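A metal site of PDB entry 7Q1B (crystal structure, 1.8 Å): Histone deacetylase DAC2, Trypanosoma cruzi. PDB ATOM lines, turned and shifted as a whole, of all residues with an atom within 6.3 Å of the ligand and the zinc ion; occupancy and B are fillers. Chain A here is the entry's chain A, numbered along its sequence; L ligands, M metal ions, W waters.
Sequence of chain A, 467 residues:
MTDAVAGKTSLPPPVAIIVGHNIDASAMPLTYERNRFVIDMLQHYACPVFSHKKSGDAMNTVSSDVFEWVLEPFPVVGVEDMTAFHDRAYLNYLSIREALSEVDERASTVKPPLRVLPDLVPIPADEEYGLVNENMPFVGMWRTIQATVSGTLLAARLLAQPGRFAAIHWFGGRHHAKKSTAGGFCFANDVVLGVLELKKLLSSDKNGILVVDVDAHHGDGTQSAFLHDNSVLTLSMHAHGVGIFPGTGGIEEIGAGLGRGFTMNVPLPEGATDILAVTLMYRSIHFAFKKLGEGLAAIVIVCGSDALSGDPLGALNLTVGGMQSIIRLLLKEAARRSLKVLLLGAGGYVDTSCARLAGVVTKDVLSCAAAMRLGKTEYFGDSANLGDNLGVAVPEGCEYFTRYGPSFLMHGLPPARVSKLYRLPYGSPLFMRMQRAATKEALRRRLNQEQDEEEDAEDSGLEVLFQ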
ATOM      1  N   GLU A 134     -23.717 -20.915  11.331  1.00  0.00           N
ATOM      2  CA  GLU A 134     -22.834 -20.408  10.278  1.00  0.00           C
ATOM      3  C   GLU A 134     -21.389 -20.259  10.747  1.00  0.00           C
ATOM      4  O   GLU A 134     -20.494 -20.083   9.910  1.00  0.00           O
ATOM      5  CB  GLU A 134     -23.359 -19.072   9.731  1.00  0.00           C
ATOM      6  CG  GLU A 134     -23.136 -17.859  10.634  1.00  0.00           C
ATOM      7  CD  GLU A 134     -24.227 -17.681  11.693  1.00  0.00           C
ATOM      8  OE1 GLU A 134     -25.139 -18.533  11.750  1.00  0.00           O
ATOM      9  OE2 GLU A 134     -24.166 -16.681  12.457  1.00  0.00           O
ATOM     10  N   HIS A 175     -16.374  -8.188   9.553  1.00  0.00           N
ATOM     11  CA  HIS A 175     -16.944  -7.121  10.358  1.00  0.00           C
ATOM     12  C   HIS A 175     -17.965  -7.571  11.406  1.00  0.00           C
ATOM     13  O   HIS A 175     -18.357  -6.734  12.225  1.00  0.00           O
ATOM     14  CB  HIS A 175     -17.593  -6.061   9.447  1.00  0.00           C
ATOM     15  CG  HIS A 175     -18.737  -6.578   8.627  1.00  0.00           C
ATOM     16  ND1 HIS A 175     -19.650  -5.735   8.025  1.00  0.00           N
ATOM     17  CD2 HIS A 175     -19.097  -7.833   8.280  1.00  0.00           C
ATOM     18  CE1 HIS A 175     -20.534  -6.463   7.361  1.00  0.00           C
ATOM     19  NE2 HIS A 175     -20.221  -7.732   7.494  1.00  0.00           N
ATOM     20  N   HIS A 176     -18.413  -8.829  11.409  1.00  0.00           N
ATOM     21  CA  HIS A 176     -19.419  -9.269  12.388  1.00  0.00           C
ATOM     22  C   HIS A 176     -18.830  -9.761  13.707  1.00  0.00           C
ATOM     23  O   HIS A 176     -19.574  -9.882  14.680  1.00  0.00           O
ATOM     24  CB  HIS A 176     -20.286 -10.407  11.833  1.00  0.00           C
ATOM     25  CG  HIS A 176     -21.238  -9.991  10.740  1.00  0.00           C
ATOM     26  ND1 HIS A 176     -22.155  -8.976  10.890  1.00  0.00           N
ATOM     27  CD2 HIS A 176     -21.431 -10.494   9.497  1.00  0.00           C
ATOM     28  CE1 HIS A 176     -22.864  -8.850   9.778  1.00  0.00           C
ATOM     29  NE2 HIS A 176     -22.439  -9.758   8.920  1.00  0.00           N
ATOM     30  N   GLY A 183     -19.765 -14.538  14.650  1.00  0.00           N
ATOM     31  CA  GLY A 183     -21.051 -14.283  14.043  1.00  0.00           C
ATOM     32  C   GLY A 183     -20.899 -14.028  12.553  1.00  0.00           C
ATOM     33  O   GLY A 183     -19.871 -13.500  12.130  1.00  0.00           O
ATOM     34  N   GLY A 184     -21.899 -14.420  11.771  1.00  0.00           N
ATOM     35  CA  GLY A 184     -21.934 -14.065  10.343  1.00  0.00           C
ATOM     36  C   GLY A 184     -20.706 -14.500   9.557  1.00  0.00           C
ATOM     37  O   GLY A 184     -20.242 -13.766   8.680  1.00  0.00           O
ATOM     38  N   PHE A 185     -20.172 -15.698   9.862  1.00  0.00           N
ATOM     39  CA  PHE A 185     -18.958 -16.275   9.275  1.00  0.00           C
ATOM     40  C   PHE A 185     -17.682 -15.600   9.757  1.00  0.00           C
ATOM     41  O   PHE A 185     -16.612 -15.836   9.170  1.00  0.00           O
ATOM     42  CB  PHE A 185     -18.934 -16.258   7.736  1.00  0.00           C
ATOM     43  CG  PHE A 185     -20.221 -16.707   7.054  1.00  0.00           C
ATOM     44  CD1 PHE A 185     -20.719 -17.977   7.252  1.00  0.00           C
ATOM     45  CD2 PHE A 185     -20.869 -15.867   6.165  1.00  0.00           C
ATOM     46  CE1 PHE A 185     -21.880 -18.389   6.607  1.00  0.00           C
ATOM     47  CE2 PHE A 185     -22.036 -16.273   5.509  1.00  0.00           C
ATOM     48  CZ  PHE A 185     -22.535 -17.533   5.737  1.00  0.00           C
ATOM     49  N   CYS A 186     -17.750 -14.750  10.776  1.00  0.00           N
ATOM     50  CA  CYS A 186     -16.601 -13.974  11.253  1.00  0.00           C
ATOM     51  C   CYS A 186     -16.163 -14.471  12.619  1.00  0.00           C
ATOM     52  O   CYS A 186     -16.988 -14.597  13.542  1.00  0.00           O
ATOM     53  CB  CYS A 186     -16.932 -12.490  11.341  1.00  0.00           C
ATOM     54  SG  CYS A 186     -17.452 -11.808   9.720  1.00  0.00           S
ATOM     55  N   ASP A 215     -20.893  -3.309   2.865  1.00  0.00           N
ATOM     56  CA  ASP A 215     -21.486  -4.641   2.837  1.00  0.00           C
ATOM     57  C   ASP A 215     -22.981  -4.530   3.115  1.00  0.00           C
ATOM     58  O   ASP A 215     -23.434  -3.617   3.812  1.00  0.00           O
ATOM     59  CB  ASP A 215     -20.751  -5.504   3.872  1.00  0.00           C
ATOM     60  CG  ASP A 215     -21.287  -6.912   3.986  1.00  0.00           C
ATOM     61  OD1 ASP A 215     -22.413  -7.076   4.458  1.00  0.00           O
ATOM     62  OD2 ASP A 215     -20.555  -7.884   3.635  1.00  0.00           O
ATOM     63  N   ALA A 216     -23.773  -5.474   2.577  1.00  0.00           N
ATOM     64  CA  ALA A 216     -25.236  -5.439   2.660  1.00  0.00           C
ATOM     65  C   ALA A 216     -25.766  -5.682   4.071  1.00  0.00           C
ATOM     66  O   ALA A 216     -26.986  -5.534   4.278  1.00  0.00           O
ATOM     67  CB  ALA A 216     -25.863  -6.501   1.756  1.00  0.00           C
ATOM     68  N   HIS A 217     -24.923  -6.093   5.003  1.00  0.00           N
ATOM     69  CA  HIS A 217     -25.372  -6.403   6.354  1.00  0.00           C
ATOM     70  C   HIS A 217     -24.769  -5.436   7.351  1.00  0.00           C
ATOM     71  O   HIS A 217     -23.714  -4.854   7.127  1.00  0.00           O
ATOM     72  CB  HIS A 217     -25.010  -7.857   6.715  1.00  0.00           C
ATOM     73  CG  HIS A 217     -25.562  -8.853   5.732  1.00  0.00           C
ATOM     74  ND1 HIS A 217     -24.861  -9.254   4.613  1.00  0.00           N
ATOM     75  CD2 HIS A 217     -26.766  -9.460   5.664  1.00  0.00           C
ATOM     76  CE1 HIS A 217     -25.591 -10.111   3.920  1.00  0.00           C
ATOM     77  NE2 HIS A 217     -26.755 -10.239   4.536  1.00  0.00           N
ATOM     78  N   HIS A 218     -25.466  -5.256   8.472  1.00  0.00           N
ATOM     79  CA  HIS A 218     -25.025  -4.304   9.482  1.00  0.00           C
ATOM     80  C   HIS A 218     -23.631  -4.670   9.998  1.00  0.00           C
ATOM     81  O   HIS A 218     -23.390  -5.804  10.404  1.00  0.00           O
ATOM     82  CB  HIS A 218     -26.018  -4.293  10.646  1.00  0.00           C
ATOM     83  CG  HIS A 218     -25.638  -3.369  11.746  1.00  0.00           C
ATOM     84  ND1 HIS A 218     -25.860  -3.651  13.078  1.00  0.00           N
ATOM     85  CD2 HIS A 218     -25.054  -2.150  11.715  1.00  0.00           C
ATOM     86  CE1 HIS A 218     -25.426  -2.657  13.816  1.00  0.00           C
ATOM     87  NE2 HIS A 218     -24.939  -1.722  13.016  1.00  0.00           N
ATOM     88  N   GLY A 241     -34.650  -5.204   8.318  1.00  0.00           N
ATOM     89  CA  GLY A 241     -36.039  -5.606   8.371  1.00  0.00           C
ATOM     90  C   GLY A 241     -36.167  -7.036   8.850  1.00  0.00           C
ATOM     91  O   GLY A 241     -35.186  -7.703   9.160  1.00  0.00           O
ATOM     92  N   VAL A 242     -37.423  -7.490   8.896  1.00  0.00           N
ATOM     93  CA  VAL A 242     -37.735  -8.816   9.388  1.00  0.00           C
ATOM     94  C   VAL A 242     -37.019  -9.864   8.544  1.00  0.00           C
ATOM     95  O   VAL A 242     -37.101  -9.856   7.310  1.00  0.00           O
ATOM     96  CB  VAL A 242     -39.254  -9.044   9.380  1.00  0.00           C
ATOM     97  CG1 VAL A 242     -39.578 -10.515   9.588  1.00  0.00           C
ATOM     98  CG2 VAL A 242     -39.918  -8.180  10.441  1.00  0.00           C
ATOM     99  N   GLY A 243     -36.299 -10.757   9.216  1.00  0.00           N
ATOM    100  CA  GLY A 243     -35.595 -11.816   8.525  1.00  0.00           C
ATOM    101  C   GLY A 243     -34.273 -11.429   7.912  1.00  0.00           C
ATOM    102  O   GLY A 243     -33.658 -12.254   7.228  1.00  0.00           O
ATOM    103  N   ILE A 244     -33.795 -10.200   8.144  1.00  0.00           N
ATOM    104  CA  ILE A 244     -32.550  -9.719   7.559  1.00  0.00           C
ATOM    105  C   ILE A 244     -31.465  -9.737   8.630  1.00  0.00           C
ATOM    106  O   ILE A 244     -31.500  -8.953   9.578  1.00  0.00           O
ATOM    107  CB  ILE A 244     -32.720  -8.330   6.939  1.00  0.00           C
ATOM    108  CG1 ILE A 244     -33.705  -8.416   5.773  1.00  0.00           C
ATOM    109  CG2 ILE A 244     -31.363  -7.799   6.481  1.00  0.00           C
ATOM    110  CD1 ILE A 244     -34.002  -7.101   5.107  1.00  0.00           C
ATOM    111  N   PHE A 245     -30.489 -10.628   8.447  1.00  0.00           N
ATOM    112  CA  PHE A 245     -29.361 -10.762   9.360  1.00  0.00           C
ATOM    113  C   PHE A 245     -28.541  -9.465   9.371  1.00  0.00           C
ATOM    114  O   PHE A 245     -28.349  -8.851   8.313  1.00  0.00           O
ATOM    115  CB  PHE A 245     -28.502 -11.949   8.918  1.00  0.00           C
ATOM    116  CG  PHE A 245     -27.322 -12.235   9.810  1.00  0.00           C
ATOM    117  CD1 PHE A 245     -27.461 -13.016  10.951  1.00  0.00           C
ATOM    118  CD2 PHE A 245     -26.063 -11.747   9.485  1.00  0.00           C
ATOM    119  CE1 PHE A 245     -26.368 -13.288  11.771  1.00  0.00           C
ATOM    120  CE2 PHE A 245     -24.973 -12.015  10.283  1.00  0.00           C
ATOM    121  CZ  PHE A 245     -25.117 -12.780  11.433  1.00  0.00           C
ATOM    122  N   PRO A 246     -28.031  -9.021  10.538  1.00  0.00           N
ATOM    123  CA  PRO A 246     -28.173  -9.682  11.847  1.00  0.00           C
ATOM    124  C   PRO A 246     -29.281  -9.098  12.736  1.00  0.00           C
ATOM    125  O   PRO A 246     -29.297  -9.397  13.943  1.00  0.00           O
ATOM    126  CB  PRO A 246     -26.811  -9.427  12.496  1.00  0.00           C
ATOM    127  CG  PRO A 246     -26.478  -8.046  12.037  1.00  0.00           C
ATOM    128  CD  PRO A 246     -27.047  -7.924  10.609  1.00  0.00           C
ATOM    129  N   GLY A 247     -30.169  -8.292  12.173  1.00  0.00           N
ATOM    130  CA  GLY A 247     -31.314  -7.788  12.914  1.00  0.00           C
ATOM    131  C   GLY A 247     -31.094  -6.475  13.646  1.00  0.00           C
ATOM    132  O   GLY A 247     -32.064  -5.931  14.210  1.00  0.00           O
ATOM    133  N   GLY A 304     -18.102  -4.733   0.887  1.00  0.00           N
ATOM    134  CA  GLY A 304     -18.674  -6.015   0.553  1.00  0.00           C
ATOM    135  C   GLY A 304     -19.570  -5.933  -0.673  1.00  0.00           C
ATOM    136  O   GLY A 304     -20.490  -5.104  -0.730  1.00  0.00           O
ATOM    137  N   ASP A 306     -21.855  -7.993  -1.504  1.00  0.00           N
ATOM    138  CA  ASP A 306     -23.147  -8.645  -1.394  1.00  0.00           C
ATOM    139  C   ASP A 306     -24.308  -7.659  -1.404  1.00  0.00           C
ATOM    140  O   ASP A 306     -25.462  -8.098  -1.397  1.00  0.00           O
ATOM    141  CB  ASP A 306     -23.214  -9.536  -0.127  1.00  0.00           C
ATOM    142  CG  ASP A 306     -22.863  -8.816   1.142  1.00  0.00           C
ATOM    143  OD1 ASP A 306     -22.520  -7.613   1.117  1.00  0.00           O
ATOM    144  OD2 ASP A 306     -22.943  -9.490   2.189  1.00  0.00           O
ATOM    145  N   LEU A 313     -27.279 -13.839  -0.590  1.00  0.00           N
ATOM    146  CA  LEU A 313     -27.354 -13.613   0.851  1.00  0.00           C
ATOM    147  C   LEU A 313     -27.565 -12.157   1.227  1.00  0.00           C
ATOM    148  O   LEU A 313     -28.152 -11.886   2.267  1.00  0.00           O
ATOM    149  CB  LEU A 313     -26.098 -14.126   1.568  1.00  0.00           C
ATOM    150  CG  LEU A 313     -25.782 -15.613   1.384  1.00  0.00           C
ATOM    151  CD1 LEU A 313     -24.620 -16.073   2.261  1.00  0.00           C
ATOM    152  CD2 LEU A 313     -27.029 -16.433   1.647  1.00  0.00           C
ATOM    153  N   GLY A 314     -27.056 -11.226   0.432  1.00  0.00           N
ATOM    154  CA  GLY A 314     -27.455  -9.837   0.581  1.00  0.00           C
ATOM    155  C   GLY A 314     -28.862  -9.615   0.071  1.00  0.00           C
ATOM    156  O   GLY A 314     -29.399 -10.408  -0.703  1.00  0.00           O
ATOM    157  N   ALA A 346     -15.334  -7.754   2.283  1.00  0.00           N
ATOM    158  CA  ALA A 346     -16.293  -8.245   3.276  1.00  0.00           C
ATOM    159  C   ALA A 346     -17.088  -9.394   2.667  1.00  0.00           C
ATOM    160  O   ALA A 346     -16.503 -10.340   2.115  1.00  0.00           O
ATOM    161  CB  ALA A 346     -17.236  -7.140   3.775  1.00  0.00           C
ATOM    162  N   GLY A 347     -18.408  -9.330   2.751  1.00  0.00           N
ATOM    163  CA  GLY A 347     -19.262 -10.330   2.129  1.00  0.00           C
ATOM    164  C   GLY A 347     -19.248 -10.219   0.614  1.00  0.00           C
ATOM    165  O   GLY A 347     -18.609  -9.352   0.019  1.00  0.00           O
ATOM    166  N   GLY A 348     -19.984 -11.129  -0.026  1.00  0.00           N
ATOM    167  CA  GLY A 348     -20.065 -11.180  -1.483  1.00  0.00           C
ATOM    168  C   GLY A 348     -20.144 -12.629  -1.938  1.00  0.00           C
ATOM    169  O   GLY A 348     -19.166 -13.368  -1.831  1.00  0.00           O
ATOM    170  N   TYR A 349     -21.308 -13.044  -2.439  1.00  0.00           N
ATOM    171  CA  TYR A 349     -21.575 -14.465  -2.662  1.00  0.00           C
ATOM    172  C   TYR A 349     -21.848 -14.787  -4.129  1.00  0.00           C
ATOM    173  O   TYR A 349     -22.432 -15.833  -4.437  1.00  0.00           O
ATOM    174  CB  TYR A 349     -22.708 -14.900  -1.733  1.00  0.00           C
ATOM    175  CG  TYR A 349     -22.266 -14.565  -0.309  1.00  0.00           C
ATOM    176  CD1 TYR A 349     -21.375 -15.376   0.368  1.00  0.00           C
ATOM    177  CD2 TYR A 349     -22.672 -13.383   0.292  1.00  0.00           C
ATOM    178  CE1 TYR A 349     -20.930 -15.051   1.660  1.00  0.00           C
ATOM    179  CE2 TYR A 349     -22.231 -13.039   1.562  1.00  0.00           C
ATOM    180  CZ  TYR A 349     -21.368 -13.866   2.244  1.00  0.00           C
ATOM    181  OH  TYR A 349     -20.957 -13.511   3.505  1.00  0.00           O
HETATM  182  N1  LIG L   1     -22.363 -10.666   6.435  1.00  0.00           N
HETATM  183  O1  LIG L   1     -22.443 -11.356   4.292  1.00  0.00           O
HETATM  184  C1  LIG L   1     -25.081 -14.702   6.801  1.00  0.00           C
HETATM  185  C2  LIG L   1     -23.485 -12.709   5.939  1.00  0.00           C
HETATM  186  C3  LIG L   1     -24.567 -13.184   5.204  1.00  0.00           C
HETATM  187  C4  LIG L   1     -26.950 -16.292   6.423  1.00  0.00           C
HETATM  188  N2  LIG L   1     -25.839 -15.745   7.213  1.00  0.00           N
HETATM  189  C5  LIG L   1     -25.757 -16.293   8.569  1.00  0.00           C
HETATM  190  C6  LIG L   1     -30.593 -13.500  12.777  1.00  0.00           C
HETATM  191  C7  LIG L   1     -22.695 -11.531   5.476  1.00  0.00           C
HETATM  192  O2  LIG L   1     -21.818  -9.421   6.146  1.00  0.00           O
HETATM  193  N3  LIG L   1     -24.071 -14.334   7.618  1.00  0.00           N
HETATM  194  C8  LIG L   1     -23.296 -13.350   7.162  1.00  0.00           C
HETATM  195  N4  LIG L   1     -25.378 -14.162   5.621  1.00  0.00           N
HETATM  196  C9  LIG L   1     -28.292 -15.938   7.053  1.00  0.00           C
HETATM  197  C10 LIG L   1     -27.099 -16.850   9.043  1.00  0.00           C
HETATM  198  C11 LIG L   1     -28.285 -16.017   8.583  1.00  0.00           C
HETATM  199  C12 LIG L   1     -29.585 -16.601   9.108  1.00  0.00           C
HETATM  200  N5  LIG L   1     -29.447 -17.129  10.467  1.00  0.00           N
HETATM  201  C13 LIG L   1     -30.628 -16.942  11.308  1.00  0.00           C
HETATM  202  C14 LIG L   1     -30.453 -15.659  12.063  1.00  0.00           C
HETATM  203  N6  LIG L   1     -29.737 -14.189  13.604  1.00  0.00           N
HETATM  204  C15 LIG L   1     -29.669 -15.485  13.165  1.00  0.00           C
HETATM  205  C16 LIG L   1     -31.057 -14.387  11.799  1.00  0.00           C
HETATM  206  C17 LIG L   1     -31.934 -13.919  10.825  1.00  0.00           C
HETATM  207  C18 LIG L   1     -32.348 -12.591  10.850  1.00  0.00           C
HETATM  208  C19 LIG L   1     -31.884 -11.731  11.840  1.00  0.00           C
HETATM  209  C20 LIG L   1     -31.003 -12.177  12.814  1.00  0.00           C
HETATM  210  C21 LIG L   1     -29.003 -13.633  14.726  1.00  0.00           C
HETATM  211 ZN    ZN M   1     -22.620  -9.196   4.246  1.00  0.00          ZN
HETATM  212  O   HOH W   1     -28.183 -13.449   4.742  1.00  0.00           O
HETATM  213  O   HOH W   2     -27.841 -19.324  11.018  1.00  0.00           O
HETATM  214  O   HOH W   3     -29.797 -15.617   4.034  1.00  0.00           O
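A ring nitrogen (NE2) of His 176 is in hydrogen-bond range of a nitrogen (N1) of the ligand (2.6 Å). An oxygen (O2) of the ligand sits close to a ring nitrogen (NE2) of His 175 (2.7 Å). An oxygen (O1) of the ligand sits close to the side-chain hydroxyl (OH) of Tyr 349 (2.7 Å).
The side-chain carboxylate (OD2) of Asp 215 sits close to the backbone NH (N) of Gly 347, 2.7 Å away. NE2 of His 217 sits at hydrogen-bond distance from O of Leu 313 (3.1 Å). NE2 of His 176 lies within hydrogen-bond range of NE2 of His 175, 3.3 Å away. A ring nitrogen (ND1) of His 176 sits close to the backbone carbonyl oxygen (O) of His 218 (3.4 Å). SG of Cys 186 sits at hydrogen-bond distance from N of His 176. The side-chain sulfur (SG) of Cys 186 sits at hydrogen-bond distance from the backbone NH (N) of His 175, at 3.8 Å. The side-chain carboxylate (OE2) of Glu 134 sits at hydrogen-bond distance from the backbone NH (N) of Gly 184 (3.3 Å). The side-chain sulfur (SG) of Cys 186 sits at hydrogen-bond distance from the backbone carbonyl oxygen (O) of Gly 184 (3.6 Å).
Glu 134 touches the ligand (CG to C5, 3.7 Å). Gly 184 touches the ligand. Phe 185 touches the ligand (CE2 to N3, 3.5 Å). Gly 243 touches the ligand (C to C18, 3.7 Å). Ile 244 touches the ligand. Phe 245 touches the ligand (N to C18, 3.6 Å). Pro 246 touches the ligand (O to C20, 3.5 Å). Gly 247 touches the ligand. Leu 313 touches the ligand. Gly 347 touches the ligand. Hydrophobic or aromatic side chains within 4 Å of the ligand: His 175, His 176, Phe 185, His 217, Phe 245, Leu 313 and Tyr 349. The nearest printed residue that does not touch the ligand is Gly 348 (5.0 Å).
Within 4 Å of the zinc ion: Asp 215, His 217 and Asp 306. Along chain A the residues within 4 Å of the zinc ion span positions 215 to 306.
The zinc ion is bound by O2 of the ligand (2.1 Å), OD2 of Asp 306 (2.1 Å), OD1 of Asp 215 (2.1 Å), O1 of the ligand (2.2 Å), ND1 of His 217 (2.3 Å) and OD2 of Asp 215 (2.5 Å).
Water W2 bridges N5 of the ligand (2.8 Å) and OE1 of Glu 134 (2.9 Å). Water W1 bridges O of Leu 313 and N4 of the ligand.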
